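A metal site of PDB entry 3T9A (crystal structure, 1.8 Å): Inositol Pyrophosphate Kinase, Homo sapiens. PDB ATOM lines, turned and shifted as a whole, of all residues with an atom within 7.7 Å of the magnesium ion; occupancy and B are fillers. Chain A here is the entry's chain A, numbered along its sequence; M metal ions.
OG1 of Thr 268 is in hydrogen-bond range of O of Ile 86 (2.7 Å). The backbone NH (N) of Gln 267 is in hydrogen-bond range of the backbone carbonyl oxygen (O) of Cys 262, at 3.1 Å. NE2 of Gln 267 is in hydrogen-bond range of OD1 of Asn 87 (2.9 Å). OD1 of Asn 87 lies close to O of Val 269 (2.9 Å). O of Thr 268 sits close to N of Gly 217 (2.8 Å). The backbone NH (N) of Thr 215 lies within hydrogen-bond range of the backbone carbonyl oxygen (O) of Cys 270. The side-chain amide nitrogen (ND2) of Asn 87 lies close to the backbone NH (N) of Thr 268. The backbone carbonyl oxygen of Phe 265 lies close to the side-chain amide oxygen of Gln 267 (2.9 Å).
Merely in contact with the magnesium ion: Cys 270 and Val 269. Of the 24 residues printed, 6 come within 4 Å of the magnesium ion.
The magnesium ion is bound by the side-chain hydroxyl (OG1) of Thr 215 (1.8 Å). O of Gln 267 binds the magnesium ion (2.3 Å). The magnesium ion is bound by O of Thr 268 (2.5 Å). Slightly farther from the magnesium ion lies SG of Cys 262 (2.8 Å).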
ATOM      1  N   ILE A  86       7.823  25.513   9.819  1.00  0.00           N
ATOM      2  CA  ILE A  86       7.462  25.469  11.253  1.00  0.00           C
ATOM      3  C   ILE A  86       7.288  24.020  11.766  1.00  0.00           C
ATOM      4  O   ILE A  86       7.825  23.638  12.822  1.00  0.00           O
ATOM      5  CB  ILE A  86       6.207  26.367  11.509  1.00  0.00           C
ATOM      6  CG1 ILE A  86       6.541  27.855  11.275  1.00  0.00           C
ATOM      7  CG2 ILE A  86       5.590  26.165  12.897  1.00  0.00           C
ATOM      8  CD1 ILE A  86       7.608  28.447  12.219  1.00  0.00           C
ATOM      9  N   ASN A  87       6.519  23.231  11.025  1.00  0.00           N
ATOM     10  CA  ASN A  87       6.331  21.802  11.291  1.00  0.00           C
ATOM     11  C   ASN A  87       6.925  20.990  10.144  1.00  0.00           C
ATOM     12  O   ASN A  87       6.434  21.068   9.010  1.00  0.00           O
ATOM     13  CB  ASN A  87       4.843  21.477  11.419  1.00  0.00           C
ATOM     14  CG  ASN A  87       4.292  21.670  12.838  1.00  0.00           C
ATOM     15  OD1 ASN A  87       3.608  20.784  13.377  1.00  0.00           O
ATOM     16  ND2 ASN A  87       4.544  22.836  13.420  1.00  0.00           N
ATOM     17  N   TYR A 214      -0.373  20.189  24.439  1.00  0.00           N
ATOM     18  CA  TYR A 214      -0.304  20.997  23.210  1.00  0.00           C
ATOM     19  C   TYR A 214       0.914  21.913  23.310  1.00  0.00           C
ATOM     20  O   TYR A 214       0.951  22.835  24.162  1.00  0.00           O
ATOM     21  CB  TYR A 214      -1.569  21.854  23.061  1.00  0.00           C
ATOM     22  CG  TYR A 214      -2.851  21.049  23.026  1.00  0.00           C
ATOM     23  CD1 TYR A 214      -3.423  20.539  24.204  1.00  0.00           C
ATOM     24  CD2 TYR A 214      -3.503  20.798  21.810  1.00  0.00           C
ATOM     25  CE1 TYR A 214      -4.599  19.796  24.163  1.00  0.00           C
ATOM     26  CE2 TYR A 214      -4.698  20.048  21.766  1.00  0.00           C
ATOM     27  CZ  TYR A 214      -5.222  19.555  22.942  1.00  0.00           C
ATOM     28  OH  TYR A 214      -6.392  18.817  22.922  1.00  0.00           O
ATOM     29  N   THR A 215       1.916  21.657  22.459  1.00  0.00           N
ATOM     30  CA  THR A 215       3.143  22.448  22.465  1.00  0.00           C
ATOM     31  C   THR A 215       3.076  23.536  21.401  1.00  0.00           C
ATOM     32  O   THR A 215       2.384  23.390  20.386  1.00  0.00           O
ATOM     33  CB  THR A 215       4.414  21.612  22.228  1.00  0.00           C
ATOM     34  OG1 THR A 215       4.551  21.275  20.837  1.00  0.00           O
ATOM     35  CG2 THR A 215       4.438  20.332  23.071  1.00  0.00           C
ATOM     36  N   VAL A 216       3.785  24.632  21.659  1.00  0.00           N
ATOM     37  CA  VAL A 216       4.046  25.645  20.635  1.00  0.00           C
ATOM     38  C   VAL A 216       5.512  25.957  20.829  1.00  0.00           C
ATOM     39  O   VAL A 216       5.897  26.844  21.631  1.00  0.00           O
ATOM     40  CB  VAL A 216       3.207  26.919  20.821  1.00  0.00           C
ATOM     41  CG1 VAL A 216       3.428  27.876  19.630  1.00  0.00           C
ATOM     42  CG2 VAL A 216       1.714  26.579  21.020  1.00  0.00           C
ATOM     43  N   GLY A 217       6.339  25.179  20.137  1.00  0.00           N
ATOM     44  CA  GLY A 217       7.760  25.139  20.413  1.00  0.00           C
ATOM     45  C   GLY A 217       8.030  24.335  21.679  1.00  0.00           C
ATOM     46  O   GLY A 217       7.118  23.991  22.445  1.00  0.00           O
ATOM     47  N   PRO A 218       9.311  24.010  21.905  1.00  0.00           N
ATOM     48  CA  PRO A 218       9.684  23.059  22.953  1.00  0.00           C
ATOM     49  C   PRO A 218       9.577  23.637  24.378  1.00  0.00           C
ATOM     50  O   PRO A 218       9.491  22.857  25.349  1.00  0.00           O
ATOM     51  CB  PRO A 218      11.126  22.683  22.600  1.00  0.00           C
ATOM     52  CG  PRO A 218      11.640  23.789  21.818  1.00  0.00           C
ATOM     53  CD  PRO A 218      10.464  24.382  21.057  1.00  0.00           C
ATOM     54  N   ASP A 219       9.540  24.962  24.506  1.00  0.00           N
ATOM     55  CA  ASP A 219       9.452  25.611  25.828  1.00  0.00           C
ATOM     56  C   ASP A 219       8.059  26.127  26.213  1.00  0.00           C
ATOM     57  O   ASP A 219       7.937  26.884  27.189  1.00  0.00           O
ATOM     58  CB  ASP A 219      10.476  26.752  25.903  1.00  0.00           C
ATOM     59  CG  ASP A 219      11.899  26.248  25.797  1.00  0.00           C
ATOM     60  OD1 ASP A 219      12.177  25.143  26.299  1.00  0.00           O
ATOM     61  OD2 ASP A 219      12.765  26.963  25.228  1.00  0.00           O
ATOM     62  N   TYR A 220       7.022  25.732  25.477  1.00  0.00           N
ATOM     63  CA  TYR A 220       5.654  26.083  25.844  1.00  0.00           C
ATOM     64  C   TYR A 220       4.751  24.868  25.672  1.00  0.00           C
ATOM     65  O   TYR A 220       4.659  24.308  24.588  1.00  0.00           O
ATOM     66  CB  TYR A 220       5.123  27.245  24.992  1.00  0.00           C
ATOM     67  CG  TYR A 220       3.705  27.657  25.307  1.00  0.00           C
ATOM     68  CD1 TYR A 220       2.621  27.001  24.709  1.00  0.00           C
ATOM     69  CD2 TYR A 220       3.429  28.691  26.211  1.00  0.00           C
ATOM     70  CE1 TYR A 220       1.310  27.375  24.993  1.00  0.00           C
ATOM     71  CE2 TYR A 220       2.127  29.068  26.497  1.00  0.00           C
ATOM     72  CZ  TYR A 220       1.067  28.411  25.893  1.00  0.00           C
ATOM     73  OH  TYR A 220      -0.222  28.782  26.181  1.00  0.00           O
ATOM     74  N   ALA A 258       7.402  17.033  26.991  1.00  0.00           N
ATOM     75  CA  ALA A 258       6.891  17.944  25.952  1.00  0.00           C
ATOM     76  C   ALA A 258       8.030  18.523  25.081  1.00  0.00           C
ATOM     77  O   ALA A 258       7.918  18.585  23.860  1.00  0.00           O
ATOM     78  CB  ALA A 258       6.042  19.050  26.572  1.00  0.00           C
ATOM     79  N   TRP A 259       9.106  18.956  25.740  1.00  0.00           N
ATOM     80  CA  TRP A 259      10.293  19.480  25.063  1.00  0.00           C
ATOM     81  C   TRP A 259      10.857  18.437  24.076  1.00  0.00           C
ATOM     82  O   TRP A 259      11.136  18.751  22.908  1.00  0.00           O
ATOM     83  CB  TRP A 259      11.325  19.846  26.124  1.00  0.00           C
ATOM     84  CG  TRP A 259      12.615  20.451  25.623  1.00  0.00           C
ATOM     85  CD1 TRP A 259      12.898  21.767  25.460  1.00  0.00           C
ATOM     86  CD2 TRP A 259      13.793  19.736  25.252  1.00  0.00           C
ATOM     87  NE1 TRP A 259      14.187  21.932  24.982  1.00  0.00           N
ATOM     88  CE2 TRP A 259      14.763  20.695  24.860  1.00  0.00           C
ATOM     89  CE3 TRP A 259      14.136  18.376  25.199  1.00  0.00           C
ATOM     90  CZ2 TRP A 259      16.047  20.337  24.428  1.00  0.00           C
ATOM     91  CZ3 TRP A 259      15.408  18.023  24.764  1.00  0.00           C
ATOM     92  CH2 TRP A 259      16.355  19.007  24.388  1.00  0.00           C
ATOM     93  N   VAL A 261       9.296  15.606  22.808  1.00  0.00           N
ATOM     94  CA  VAL A 261       8.377  15.229  21.746  1.00  0.00           C
ATOM     95  C   VAL A 261       8.369  16.277  20.613  1.00  0.00           C
ATOM     96  O   VAL A 261       8.467  15.929  19.439  1.00  0.00           O
ATOM     97  CB  VAL A 261       6.955  14.989  22.297  1.00  0.00           C
ATOM     98  CG1 VAL A 261       5.926  14.970  21.167  1.00  0.00           C
ATOM     99  CG2 VAL A 261       6.951  13.668  23.077  1.00  0.00           C
ATOM    100  N   CYS A 262       8.294  17.552  20.991  1.00  0.00           N
ATOM    101  CA  CYS A 262       8.325  18.656  20.025  1.00  0.00           C
ATOM    102  C   CYS A 262       9.572  18.594  19.124  1.00  0.00           C
ATOM    103  O   CYS A 262       9.492  18.688  17.886  1.00  0.00           O
ATOM    104  CB  CYS A 262       8.244  19.994  20.774  1.00  0.00           C
ATOM    105  SG  CYS A 262       8.340  21.450  19.749  1.00  0.00           S
ATOM    106  N   LEU A 263      10.732  18.443  19.757  1.00  0.00           N
ATOM    107  CA  LEU A 263      11.989  18.382  19.010  1.00  0.00           C
ATOM    108  C   LEU A 263      12.190  17.085  18.218  1.00  0.00           C
ATOM    109  O   LEU A 263      12.646  17.135  17.074  1.00  0.00           O
ATOM    110  CB  LEU A 263      13.189  18.709  19.920  1.00  0.00           C
ATOM    111  CG  LEU A 263      13.152  20.156  20.448  1.00  0.00           C
ATOM    112  CD1 LEU A 263      14.075  20.367  21.631  1.00  0.00           C
ATOM    113  CD2 LEU A 263      13.505  21.170  19.317  1.00  0.00           C
ATOM    114  N   PHE A 265      10.038  15.006  16.932  1.00  0.00           N
ATOM    115  CA  PHE A 265       9.170  14.948  15.771  1.00  0.00           C
ATOM    116  C   PHE A 265       9.265  16.193  14.879  1.00  0.00           C
ATOM    117  O   PHE A 265       8.595  16.270  13.856  1.00  0.00           O
ATOM    118  CB  PHE A 265       7.719  14.685  16.217  1.00  0.00           C
ATOM    119  CG  PHE A 265       7.512  13.304  16.771  1.00  0.00           C
ATOM    120  CD1 PHE A 265       7.205  12.238  15.931  1.00  0.00           C
ATOM    121  CD2 PHE A 265       7.679  13.053  18.134  1.00  0.00           C
ATOM    122  CE1 PHE A 265       7.035  10.942  16.447  1.00  0.00           C
ATOM    123  CE2 PHE A 265       7.518  11.761  18.651  1.00  0.00           C
ATOM    124  CZ  PHE A 265       7.185  10.706  17.806  1.00  0.00           C
ATOM    125  N   LYS A 266      10.091  17.158  15.285  1.00  0.00           N
ATOM    126  CA  LYS A 266      10.257  18.414  14.537  1.00  0.00           C
ATOM    127  C   LYS A 266       8.926  19.111  14.242  1.00  0.00           C
ATOM    128  O   LYS A 266       8.749  19.714  13.175  1.00  0.00           O
ATOM    129  CB  LYS A 266      11.016  18.151  13.228  1.00  0.00           C
ATOM    130  CG  LYS A 266      12.416  17.574  13.396  1.00  0.00           C
ATOM    131  CD  LYS A 266      13.028  17.268  12.013  1.00  0.00           C
ATOM    132  CE  LYS A 266      14.200  16.298  12.142  1.00  0.00           C
ATOM    133  NZ  LYS A 266      14.485  15.577  10.857  1.00  0.00           N
ATOM    134  N   GLN A 267       7.975  19.019  15.171  1.00  0.00           N
ATOM    135  CA  GLN A 267       6.686  19.680  14.987  1.00  0.00           C
ATOM    136  C   GLN A 267       6.553  20.803  16.003  1.00  0.00           C
ATOM    137  O   GLN A 267       6.157  20.549  17.137  1.00  0.00           O
ATOM    138  CB  GLN A 267       5.511  18.692  15.152  1.00  0.00           C
ATOM    139  CG  GLN A 267       5.580  17.423  14.296  1.00  0.00           C
ATOM    140  CD  GLN A 267       5.584  17.710  12.788  1.00  0.00           C
ATOM    141  OE1 GLN A 267       6.585  17.474  12.108  1.00  0.00           O
ATOM    142  NE2 GLN A 267       4.477  18.221  12.288  1.00  0.00           N
ATOM    143  N   THR A 268       6.880  22.035  15.619  1.00  0.00           N
ATOM    144  CA  THR A 268       6.697  23.190  16.523  1.00  0.00           C
ATOM    145  C   THR A 268       5.331  23.154  17.246  1.00  0.00           C
ATOM    146  O   THR A 268       5.257  23.204  18.470  1.00  0.00           O
ATOM    147  CB  THR A 268       6.883  24.539  15.763  1.00  0.00           C
ATOM    148  OG1 THR A 268       8.226  24.604  15.258  1.00  0.00           O
ATOM    149  CG2 THR A 268       6.598  25.754  16.677  1.00  0.00           C
ATOM    150  N   VAL A 269       4.246  23.059  16.476  1.00  0.00           N
ATOM    151  CA  VAL A 269       2.915  22.933  17.057  1.00  0.00           C
ATOM    152  C   VAL A 269       2.610  21.429  17.073  1.00  0.00           C
ATOM    153  O   VAL A 269       2.477  20.824  16.015  1.00  0.00           O
ATOM    154  CB  VAL A 269       1.851  23.687  16.206  1.00  0.00           C
ATOM    155  CG1 VAL A 269       0.443  23.547  16.836  1.00  0.00           C
ATOM    156  CG2 VAL A 269       2.236  25.167  16.012  1.00  0.00           C
ATOM    157  N   CYS A 270       2.544  20.813  18.273  1.00  0.00           N
ATOM    158  CA  CYS A 270       2.334  19.367  18.373  1.00  0.00           C
ATOM    159  C   CYS A 270       1.419  19.007  19.556  1.00  0.00           C
ATOM    160  O   CYS A 270       1.577  19.561  20.651  1.00  0.00           O
ATOM    161  CB  CYS A 270       3.692  18.654  18.531  1.00  0.00           C
ATOM    162  SG  CYS A 270       3.708  16.877  18.291  1.00  0.00           S
ATOM    163  N   GLY A 271       0.505  18.084  19.336  1.00  0.00           N
ATOM    164  CA  GLY A 271      -0.304  17.571  20.433  1.00  0.00           C
ATOM    165  C   GLY A 271       0.120  16.137  20.692  1.00  0.00           C
ATOM    166  O   GLY A 271       0.438  15.394  19.749  1.00  0.00           O
ATOM    167  N   PHE A 272       0.122  15.737  21.952  1.00  0.00           N
ATOM    168  CA  PHE A 272       0.308  14.320  22.302  1.00  0.00           C
ATOM    169  C   PHE A 272      -0.477  14.009  23.576  1.00  0.00           C
ATOM    170  O   PHE A 272      -0.913  14.925  24.266  1.00  0.00           O
ATOM    171  CB  PHE A 272       1.793  13.954  22.433  1.00  0.00           C
ATOM    172  CG  PHE A 272       2.521  14.652  23.547  1.00  0.00           C
ATOM    173  CD1 PHE A 272       3.087  15.907  23.325  1.00  0.00           C
ATOM    174  CD2 PHE A 272       2.650  14.042  24.810  1.00  0.00           C
ATOM    175  CE1 PHE A 272       3.761  16.585  24.349  1.00  0.00           C
ATOM    176  CE2 PHE A 272       3.317  14.708  25.844  1.00  0.00           C
ATOM    177  CZ  PHE A 272       3.901  15.979  25.604  1.00  0.00           C
ATOM    178  N   GLY A 288       0.800  15.240  16.162  1.00  0.00           N
ATOM    179  CA  GLY A 288       1.282  16.315  15.314  1.00  0.00           C
ATOM    180  C   GLY A 288       0.473  17.590  15.506  1.00  0.00           C
ATOM    181  O   GLY A 288      -0.092  17.813  16.576  1.00  0.00           O
ATOM    182  N   PHE A 289       0.400  18.387  14.456  1.00  0.00           N
ATOM    183  CA  PHE A 289      -0.255  19.691  14.489  1.00  0.00           C
ATOM    184  C   PHE A 289      -1.634  19.662  15.139  1.00  0.00           C
ATOM    185  O   PHE A 289      -2.560  18.973  14.661  1.00  0.00           O
ATOM    186  CB  PHE A 289      -0.338  20.315  13.102  1.00  0.00           C
ATOM    187  CG  PHE A 289      -0.496  21.796  13.119  1.00  0.00           C
ATOM    188  CD1 PHE A 289      -1.752  22.370  13.372  1.00  0.00           C
ATOM    189  CD2 PHE A 289       0.588  22.632  12.875  1.00  0.00           C
ATOM    190  CE1 PHE A 289      -1.910  23.743  13.385  1.00  0.00           C
ATOM    191  CE2 PHE A 289       0.430  24.005  12.888  1.00  0.00           C
ATOM    192  CZ  PHE A 289      -0.819  24.561  13.143  1.00  0.00           C
HETATM  193 MG    MG M   1       5.583  20.935  19.355  1.00  0.00          MG
